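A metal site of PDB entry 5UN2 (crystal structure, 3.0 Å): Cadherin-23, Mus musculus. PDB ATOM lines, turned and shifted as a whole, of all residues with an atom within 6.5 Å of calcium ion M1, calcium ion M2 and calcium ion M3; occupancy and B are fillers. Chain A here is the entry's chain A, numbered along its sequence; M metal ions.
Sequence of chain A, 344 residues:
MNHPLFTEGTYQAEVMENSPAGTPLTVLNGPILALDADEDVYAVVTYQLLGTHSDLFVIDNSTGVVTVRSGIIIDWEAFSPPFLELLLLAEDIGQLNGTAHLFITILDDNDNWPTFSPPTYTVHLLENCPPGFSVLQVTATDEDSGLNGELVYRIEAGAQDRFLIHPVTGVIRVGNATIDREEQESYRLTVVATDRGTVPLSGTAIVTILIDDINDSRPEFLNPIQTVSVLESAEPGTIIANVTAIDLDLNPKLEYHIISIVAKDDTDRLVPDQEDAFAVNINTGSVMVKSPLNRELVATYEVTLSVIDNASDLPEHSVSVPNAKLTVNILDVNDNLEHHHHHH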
ATOM      1  N   GLU A 127      25.866  -8.396 -18.304  1.00  0.00           N
ATOM      2  CA  GLU A 127      26.009  -7.206 -19.142  1.00  0.00           C
ATOM      3  C   GLU A 127      24.638  -6.704 -19.588  1.00  0.00           C
ATOM      4  O   GLU A 127      23.633  -7.423 -19.450  1.00  0.00           O
ATOM      5  CB  GLU A 127      26.932  -7.477 -20.337  1.00  0.00           C
ATOM      6  CG  GLU A 127      26.418  -8.439 -21.405  1.00  0.00           C
ATOM      7  CD  GLU A 127      27.358  -8.531 -22.600  1.00  0.00           C
ATOM      8  OE1 GLU A 127      27.789  -9.660 -22.944  1.00  0.00           O
ATOM      9  OE2 GLU A 127      27.683  -7.475 -23.212  1.00  0.00           O
ATOM     10  N   ASN A 128      24.604  -5.459 -20.111  1.00  0.00           N
ATOM     11  CA  ASN A 128      23.347  -4.737 -20.481  1.00  0.00           C
ATOM     12  C   ASN A 128      22.378  -4.579 -19.311  1.00  0.00           C
ATOM     13  O   ASN A 128      21.167  -4.500 -19.534  1.00  0.00           O
ATOM     14  CB  ASN A 128      22.582  -5.410 -21.643  1.00  0.00           C
ATOM     15  CG  ASN A 128      23.473  -5.900 -22.752  1.00  0.00           C
ATOM     16  OD1 ASN A 128      24.448  -5.254 -23.127  1.00  0.00           O
ATOM     17  ND2 ASN A 128      23.133  -7.072 -23.289  1.00  0.00           N
ATOM     18  N   ILE A 179      27.226  -1.332 -19.345  1.00  0.00           N
ATOM     19  CA  ILE A 179      28.192  -2.375 -18.922  1.00  0.00           C
ATOM     20  C   ILE A 179      28.312  -3.452 -20.014  1.00  0.00           C
ATOM     21  O   ILE A 179      27.474  -4.352 -20.091  1.00  0.00           O
ATOM     22  CB  ILE A 179      27.820  -3.049 -17.574  1.00  0.00           C
ATOM     23  CG1 ILE A 179      27.587  -1.988 -16.482  1.00  0.00           C
ATOM     24  CG2 ILE A 179      28.892  -4.073 -17.163  1.00  0.00           C
ATOM     25  CD1 ILE A 179      28.668  -0.919 -16.397  1.00  0.00           C
ATOM     26  N   ASP A 180      29.372  -3.334 -20.820  1.00  0.00           N
ATOM     27  CA  ASP A 180      29.603  -4.189 -21.998  1.00  0.00           C
ATOM     28  C   ASP A 180      30.750  -5.150 -21.734  1.00  0.00           C
ATOM     29  O   ASP A 180      31.888  -4.708 -21.549  1.00  0.00           O
ATOM     30  CB  ASP A 180      29.937  -3.303 -23.202  1.00  0.00           C
ATOM     31  CG  ASP A 180      29.997  -4.056 -24.508  1.00  0.00           C
ATOM     32  OD1 ASP A 180      29.719  -5.281 -24.525  1.00  0.00           O
ATOM     33  OD2 ASP A 180      30.277  -3.400 -25.533  1.00  0.00           O
ATOM     34  N   ARG A 181      30.474  -6.459 -21.713  1.00  0.00           N
ATOM     35  CA  ARG A 181      31.510  -7.453 -21.420  1.00  0.00           C
ATOM     36  C   ARG A 181      32.617  -7.380 -22.464  1.00  0.00           C
ATOM     37  O   ARG A 181      33.785  -7.573 -22.137  1.00  0.00           O
ATOM     38  CB  ARG A 181      30.951  -8.889 -21.363  1.00  0.00           C
ATOM     39  CG  ARG A 181      31.856  -9.871 -20.586  1.00  0.00           C
ATOM     40  CD  ARG A 181      31.656 -11.332 -20.988  1.00  0.00           C
ATOM     41  NE  ARG A 181      31.920 -11.548 -22.415  1.00  0.00           N
ATOM     42  CZ  ARG A 181      33.106 -11.793 -22.977  1.00  0.00           C
ATOM     43  NH1 ARG A 181      33.179 -11.945 -24.297  1.00  0.00           N
ATOM     44  NH2 ARG A 181      34.223 -11.897 -22.256  1.00  0.00           N
ATOM     45  N   GLU A 182      32.234  -7.072 -23.695  1.00  0.00           N
ATOM     46  CA  GLU A 182      33.188  -6.974 -24.820  1.00  0.00           C
ATOM     47  C   GLU A 182      34.117  -5.732 -24.718  1.00  0.00           C
ATOM     48  O   GLU A 182      35.230  -5.761 -25.238  1.00  0.00           O
ATOM     49  CB  GLU A 182      32.446  -7.027 -26.168  1.00  0.00           C
ATOM     50  CG  GLU A 182      31.915  -8.415 -26.551  1.00  0.00           C
ATOM     51  CD  GLU A 182      30.770  -8.951 -25.667  1.00  0.00           C
ATOM     52  OE1 GLU A 182      29.754  -8.248 -25.399  1.00  0.00           O
ATOM     53  OE2 GLU A 182      30.847 -10.124 -25.254  1.00  0.00           O
ATOM     54  N   GLU A 183      33.656  -4.676 -24.045  1.00  0.00           N
ATOM     55  CA  GLU A 183      34.430  -3.433 -23.823  1.00  0.00           C
ATOM     56  C   GLU A 183      35.279  -3.476 -22.554  1.00  0.00           C
ATOM     57  O   GLU A 183      36.333  -2.836 -22.484  1.00  0.00           O
ATOM     58  CB  GLU A 183      33.477  -2.233 -23.766  1.00  0.00           C
ATOM     59  CG  GLU A 183      34.115  -0.860 -23.999  1.00  0.00           C
ATOM     60  CD  GLU A 183      34.478  -0.104 -22.726  1.00  0.00           C
ATOM     61  OE1 GLU A 183      35.247   0.895 -22.843  1.00  0.00           O
ATOM     62  OE2 GLU A 183      34.015  -0.494 -21.633  1.00  0.00           O
ATOM     63  N   ASP A 212      29.505 -11.191 -16.706  1.00  0.00           N
ATOM     64  CA  ASP A 212      29.049 -12.401 -17.388  1.00  0.00           C
ATOM     65  C   ASP A 212      28.605 -12.032 -18.798  1.00  0.00           C
ATOM     66  O   ASP A 212      28.407 -10.853 -19.104  1.00  0.00           O
ATOM     67  CB  ASP A 212      27.895 -13.072 -16.602  1.00  0.00           C
ATOM     68  CG  ASP A 212      28.367 -13.696 -15.273  1.00  0.00           C
ATOM     69  OD1 ASP A 212      29.590 -13.716 -14.995  1.00  0.00           O
ATOM     70  OD2 ASP A 212      27.512 -14.191 -14.505  1.00  0.00           O
ATOM     71  N   ASP A 213      28.445 -13.049 -19.636  1.00  0.00           N
ATOM     72  CA  ASP A 213      28.153 -12.877 -21.064  1.00  0.00           C
ATOM     73  C   ASP A 213      26.688 -13.067 -21.432  1.00  0.00           C
ATOM     74  O   ASP A 213      26.039 -14.014 -21.002  1.00  0.00           O
ATOM     75  CB  ASP A 213      28.994 -13.872 -21.881  1.00  0.00           C
ATOM     76  CG  ASP A 213      28.861 -13.654 -23.393  1.00  0.00           C
ATOM     77  OD1 ASP A 213      29.279 -12.571 -23.895  1.00  0.00           O
ATOM     78  OD2 ASP A 213      28.364 -14.585 -24.085  1.00  0.00           O
ATOM     79  N   ILE A 214      26.198 -12.135 -22.250  1.00  0.00           N
ATOM     80  CA  ILE A 214      25.060 -12.348 -23.126  1.00  0.00           C
ATOM     81  C   ILE A 214      25.639 -12.332 -24.542  1.00  0.00           C
ATOM     82  O   ILE A 214      26.485 -11.470 -24.855  1.00  0.00           O
ATOM     83  CB  ILE A 214      24.034 -11.211 -22.980  1.00  0.00           C
ATOM     84  CG1 ILE A 214      23.594 -11.063 -21.521  1.00  0.00           C
ATOM     85  CG2 ILE A 214      22.830 -11.442 -23.882  1.00  0.00           C
ATOM     86  CD1 ILE A 214      22.441 -10.097 -21.338  1.00  0.00           C
ATOM     87  N   ASN A 215      25.238 -13.287 -25.386  1.00  0.00           N
ATOM     88  CA  ASN A 215      25.762 -13.387 -26.756  1.00  0.00           C
ATOM     89  C   ASN A 215      25.054 -12.333 -27.578  1.00  0.00           C
ATOM     90  O   ASN A 215      24.011 -12.610 -28.174  1.00  0.00           O
ATOM     91  CB  ASN A 215      25.574 -14.814 -27.308  1.00  0.00           C
ATOM     92  CG  ASN A 215      26.328 -15.066 -28.612  1.00  0.00           C
ATOM     93  OD1 ASN A 215      26.650 -14.148 -29.363  1.00  0.00           O
ATOM     94  ND2 ASN A 215      26.570 -16.346 -28.903  1.00  0.00           N
ATOM     95  N   ASP A 216      25.620 -11.123 -27.581  1.00  0.00           N
ATOM     96  CA  ASP A 216      24.939  -9.896 -28.027  1.00  0.00           C
ATOM     97  C   ASP A 216      25.748  -9.029 -29.009  1.00  0.00           C
ATOM     98  O   ASP A 216      25.406  -7.863 -29.237  1.00  0.00           O
ATOM     99  CB  ASP A 216      24.534  -9.061 -26.799  1.00  0.00           C
ATOM    100  CG  ASP A 216      25.731  -8.431 -26.072  1.00  0.00           C
ATOM    101  OD1 ASP A 216      26.912  -8.772 -26.378  1.00  0.00           O
ATOM    102  OD2 ASP A 216      25.503  -7.562 -25.185  1.00  0.00           O
ATOM    103  N   SER A 217      26.787  -9.614 -29.592  1.00  0.00           N
ATOM    104  CA  SER A 217      27.746  -8.877 -30.432  1.00  0.00           C
ATOM    105  C   SER A 217      27.946  -9.598 -31.770  1.00  0.00           C
ATOM    106  O   SER A 217      28.378 -10.760 -31.780  1.00  0.00           O
ATOM    107  CB  SER A 217      29.066  -8.749 -29.675  1.00  0.00           C
ATOM    108  OG  SER A 217      30.105  -8.364 -30.528  1.00  0.00           O
ATOM    109  N   ARG A 218      27.619  -8.912 -32.863  1.00  0.00           N
ATOM    110  CA  ARG A 218      27.580  -9.540 -34.193  1.00  0.00           C
ATOM    111  C   ARG A 218      28.960  -9.966 -34.677  1.00  0.00           C
ATOM    112  O   ARG A 218      29.951  -9.288 -34.381  1.00  0.00           O
ATOM    113  CB  ARG A 218      26.925  -8.617 -35.238  1.00  0.00           C
ATOM    114  CG  ARG A 218      27.796  -7.432 -35.679  1.00  0.00           C
ATOM    115  CD  ARG A 218      27.151  -6.606 -36.780  1.00  0.00           C
ATOM    116  NE  ARG A 218      26.002  -5.864 -36.282  1.00  0.00           N
ATOM    117  CZ  ARG A 218      24.737  -6.248 -36.369  1.00  0.00           C
ATOM    118  NH1 ARG A 218      23.804  -5.445 -35.842  1.00  0.00           N
ATOM    119  NH2 ARG A 218      24.372  -7.389 -36.967  1.00  0.00           N
ATOM    120  N   PRO A 219      29.024 -11.075 -35.430  1.00  0.00           N
ATOM    121  CA  PRO A 219      30.313 -11.439 -36.016  1.00  0.00           C
ATOM    122  C   PRO A 219      30.821 -10.360 -36.987  1.00  0.00           C
ATOM    123  O   PRO A 219      30.022  -9.639 -37.618  1.00  0.00           O
ATOM    124  CB  PRO A 219      30.016 -12.744 -36.741  1.00  0.00           C
ATOM    125  CG  PRO A 219      28.570 -12.649 -37.076  1.00  0.00           C
ATOM    126  CD  PRO A 219      27.956 -11.978 -35.886  1.00  0.00           C
ATOM    127  N   ASP A 247      33.583 -13.216 -33.642  1.00  0.00           N
ATOM    128  CA  ASP A 247      32.508 -12.831 -32.723  1.00  0.00           C
ATOM    129  C   ASP A 247      33.183 -12.679 -31.349  1.00  0.00           C
ATOM    130  O   ASP A 247      33.882 -13.580 -30.897  1.00  0.00           O
ATOM    131  CB  ASP A 247      31.426 -13.948 -32.700  1.00  0.00           C
ATOM    132  CG  ASP A 247      30.047 -13.506 -32.099  1.00  0.00           C
ATOM    133  OD1 ASP A 247      29.853 -13.463 -30.869  1.00  0.00           O
ATOM    134  OD2 ASP A 247      29.097 -13.262 -32.890  1.00  0.00           O
ATOM    135  N   LEU A 248      32.999 -11.541 -30.691  1.00  0.00           N
ATOM    136  CA  LEU A 248      33.723 -11.287 -29.438  1.00  0.00           C
ATOM    137  C   LEU A 248      33.004 -11.837 -28.213  1.00  0.00           C
ATOM    138  O   LEU A 248      33.492 -11.649 -27.103  1.00  0.00           O
ATOM    139  CB  LEU A 248      34.008  -9.786 -29.255  1.00  0.00           C
ATOM    140  CG  LEU A 248      34.718  -9.091 -30.421  1.00  0.00           C
ATOM    141  CD1 LEU A 248      34.761  -7.586 -30.257  1.00  0.00           C
ATOM    142  CD2 LEU A 248      36.123  -9.639 -30.616  1.00  0.00           C
ATOM    143  N   ASP A 249      31.863 -12.517 -28.412  1.00  0.00           N
ATOM    144  CA  ASP A 249      31.094 -13.127 -27.296  1.00  0.00           C
ATOM    145  C   ASP A 249      31.732 -14.444 -26.856  1.00  0.00           C
ATOM    146  O   ASP A 249      32.654 -14.935 -27.509  1.00  0.00           O
ATOM    147  CB  ASP A 249      29.640 -13.374 -27.696  1.00  0.00           C
ATOM    148  CG  ASP A 249      28.920 -12.123 -28.086  1.00  0.00           C
ATOM    149  OD1 ASP A 249      28.894 -11.202 -27.256  1.00  0.00           O
ATOM    150  OD2 ASP A 249      28.371 -12.070 -29.206  1.00  0.00           O
ATOM    151  N   LEU A 250      31.215 -15.032 -25.790  1.00  0.00           N
ATOM    152  CA  LEU A 250      31.935 -16.109 -25.115  1.00  0.00           C
ATOM    153  C   LEU A 250      31.909 -17.477 -25.802  1.00  0.00           C
ATOM    154  O   LEU A 250      32.903 -18.208 -25.745  1.00  0.00           O
ATOM    155  CB  LEU A 250      31.499 -16.227 -23.660  1.00  0.00           C
ATOM    156  CG  LEU A 250      32.627 -16.403 -22.647  1.00  0.00           C
ATOM    157  CD1 LEU A 250      33.628 -15.254 -22.727  1.00  0.00           C
ATOM    158  CD2 LEU A 250      32.032 -16.525 -21.246  1.00  0.00           C
ATOM    159  N   PRO A 252      30.628 -18.570 -29.401  1.00  0.00           N
ATOM    160  CA  PRO A 252      29.949 -18.406 -30.693  1.00  0.00           C
ATOM    161  C   PRO A 252      29.875 -19.696 -31.462  1.00  0.00           C
ATOM    162  O   PRO A 252      30.701 -20.565 -31.260  1.00  0.00           O
ATOM    163  CB  PRO A 252      30.839 -17.407 -31.438  1.00  0.00           C
ATOM    164  CG  PRO A 252      31.933 -17.028 -30.506  1.00  0.00           C
ATOM    165  CD  PRO A 252      32.011 -18.093 -29.469  1.00  0.00           C
ATOM    166  N   LEU A 254      29.811 -19.893 -35.263  1.00  0.00           N
ATOM    167  CA  LEU A 254      29.782 -19.219 -36.556  1.00  0.00           C
ATOM    168  C   LEU A 254      29.454 -20.144 -37.704  1.00  0.00           C
ATOM    169  O   LEU A 254      29.912 -21.272 -37.755  1.00  0.00           O
ATOM    170  CB  LEU A 254      31.090 -18.492 -36.841  1.00  0.00           C
ATOM    171  CG  LEU A 254      31.177 -17.045 -36.328  1.00  0.00           C
ATOM    172  CD1 LEU A 254      30.707 -16.954 -34.880  1.00  0.00           C
ATOM    173  CD2 LEU A 254      32.598 -16.508 -36.471  1.00  0.00           C
ATOM    174  N   ASP A 309      26.199 -15.829 -36.050  1.00  0.00           N
ATOM    175  CA  ASP A 309      26.396 -16.512 -34.781  1.00  0.00           C
ATOM    176  C   ASP A 309      25.077 -17.192 -34.349  1.00  0.00           C
ATOM    177  O   ASP A 309      24.176 -16.515 -33.852  1.00  0.00           O
ATOM    178  CB  ASP A 309      26.883 -15.534 -33.704  1.00  0.00           C
ATOM    179  CG  ASP A 309      27.357 -16.225 -32.425  1.00  0.00           C
ATOM    180  OD1 ASP A 309      27.255 -17.473 -32.356  1.00  0.00           O
ATOM    181  OD2 ASP A 309      27.844 -15.519 -31.509  1.00  0.00           O
ATOM    182  N   ALA A 311      24.540 -19.033 -31.871  1.00  0.00           N
ATOM    183  CA  ALA A 311      24.368 -18.938 -30.431  1.00  0.00           C
ATOM    184  C   ALA A 311      23.884 -17.563 -29.964  1.00  0.00           C
ATOM    185  O   ALA A 311      23.610 -17.407 -28.777  1.00  0.00           O
ATOM    186  CB  ALA A 311      25.665 -19.297 -29.726  1.00  0.00           C
ATOM    187  N   SER A 312      23.773 -16.568 -30.851  1.00  0.00           N
ATOM    188  CA  SER A 312      23.500 -15.205 -30.393  1.00  0.00           C
ATOM    189  C   SER A 312      22.115 -15.071 -29.717  1.00  0.00           C
ATOM    190  O   SER A 312      21.098 -15.561 -30.219  1.00  0.00           O
ATOM    191  CB  SER A 312      23.702 -14.141 -31.483  1.00  0.00           C
ATOM    192  OG  SER A 312      22.564 -14.016 -32.318  1.00  0.00           O
ATOM    193  N   ASP A 313      22.130 -14.429 -28.547  1.00  0.00           N
ATOM    194  CA  ASP A 313      20.946 -14.258 -27.733  1.00  0.00           C
ATOM    195  C   ASP A 313      20.100 -13.098 -28.293  1.00  0.00           C
ATOM    196  O   ASP A 313      18.915 -13.092 -28.098  1.00  0.00           O
ATOM    197  CB  ASP A 313      21.316 -14.025 -26.255  1.00  0.00           C
ATOM    198  CG  ASP A 313      21.956 -15.268 -25.574  1.00  0.00           C
ATOM    199  OD1 ASP A 313      21.426 -16.393 -25.681  1.00  0.00           O
ATOM    200  OD2 ASP A 313      23.003 -15.125 -24.891  1.00  0.00           O
ATOM    201  N   HIS A 317      21.812  -8.791 -33.661  1.00  0.00           N
ATOM    202  CA  HIS A 317      23.289  -8.905 -33.705  1.00  0.00           C
ATOM    203  C   HIS A 317      23.739 -10.325 -34.038  1.00  0.00           C
ATOM    204  O   HIS A 317      24.647 -10.905 -33.397  1.00  0.00           O
ATOM    205  CB  HIS A 317      23.858  -8.460 -32.371  1.00  0.00           C
ATOM    206  CG  HIS A 317      23.453  -7.083 -31.996  1.00  0.00           C
ATOM    207  ND1 HIS A 317      24.156  -5.963 -32.382  1.00  0.00           N
ATOM    208  CD2 HIS A 317      22.401  -6.630 -31.267  1.00  0.00           C
ATOM    209  CE1 HIS A 317      23.562  -4.886 -31.908  1.00  0.00           C
ATOM    210  NE2 HIS A 317      22.490  -5.267 -31.232  1.00  0.00           N
ATOM    211  N   SER A 318      23.071 -10.891 -35.041  1.00  0.00           N
ATOM    212  CA  SER A 318      23.262 -12.272 -35.430  1.00  0.00           C
ATOM    213  C   SER A 318      24.242 -12.370 -36.564  1.00  0.00           C
ATOM    214  O   SER A 318      25.103 -13.244 -36.574  1.00  0.00           O
ATOM    215  CB  SER A 318      21.948 -12.865 -35.910  1.00  0.00           C
ATOM    216  OG  SER A 318      21.082 -13.072 -34.830  1.00  0.00           O
HETATM  217 CA    CA M   1      27.309 -12.855 -31.297  1.00  0.00          CA
HETATM  218 CA    CA M   2      28.438 -10.394 -25.093  1.00  0.00          CA
HETATM  219 CA    CA M   3      27.970  -6.520 -25.354  1.00  0.00          CA
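The side-chain carboxylate (OD2) of Asp 216 sits close to the side-chain amide nitrogen (ND2) of Asn 128.
The side-chain carboxylate of Asp 213 lies within hydrogen-bond range of the backbone NH of Leu 250, 3.4 Å away.
OE2 of Glu 127 lies close to N of Arg 181 (3.3 Å).
The side-chain amide nitrogen of Asn 215 sits close to the backbone carbonyl oxygen of Ala 311.
The backbone NH (N) of Asp 309 lies within hydrogen-bond range of the backbone carbonyl oxygen (O) of Ser 318 (2.9 Å).
The side-chain hydroxyl (OG) of Ser 312 lies within hydrogen-bond range of the side-chain hydroxyl (OG) of Ser 318.
The guanidinium group (NE) of Arg 181 lies close to the side-chain carboxylate (OD1) of Asp 213, 3.2 Å away.
O of Asn 215 lies within hydrogen-bond range of N of Asp 313 (2.6 Å).
CB of Ser 312 touches calcium ion M1, 3.8 Å away.
His 317 touches calcium ion M1 (O to CA, 3.9 Å).
Within 4 Å of calcium ion M2: Glu 127, Glu 182, Asp 213, Ile 214, Asp 216 and Asp 249.
Of the 27 residues printed, 4 come within 4 Å of calcium ion M3.
The nearest printed residue that does not touch calcium ion M3 is Asn 128 (4.4 Å).
O of Ser 217 is bound to calcium ion M1, at 2.4 Å.
OD1 of Asn 215 binds calcium ion M1 (2.4 Å).
OD2 of Asp 247 binds calcium ion M1 (2.4 Å).
OD2 of Asp 249 binds calcium ion M1 (2.5 Å).
OD1 of Asp 247 is bound to calcium ion M1, 2.7 Å away.
The side-chain carboxylate (OD2) of Asp 309 is bound to calcium ion M1 (2.7 Å).
Calcium ion M2 is bound by O of Ile 214 (2.2 Å), OD1 of Asp 249 (2.4 Å), OE1 of Glu 127 (2.4 Å), OE2 of Glu 182 (2.4 Å), OE1 of Glu 182 (2.5 Å), OD1 of Asp 216 (2.6 Å) and OD1 of Asp 213 (2.6 Å).
Calcium ion M3 is bound by OD1 of Asp 180 (2.3 Å), OE2 of Glu 127 (2.4 Å), OE1 of Glu 182 (2.5 Å), OD2 of Asp 216 (2.7 Å) and OD1 of Asp 216 (2.7 Å).
Calcium ion M3 has five donor atoms within binding distance.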
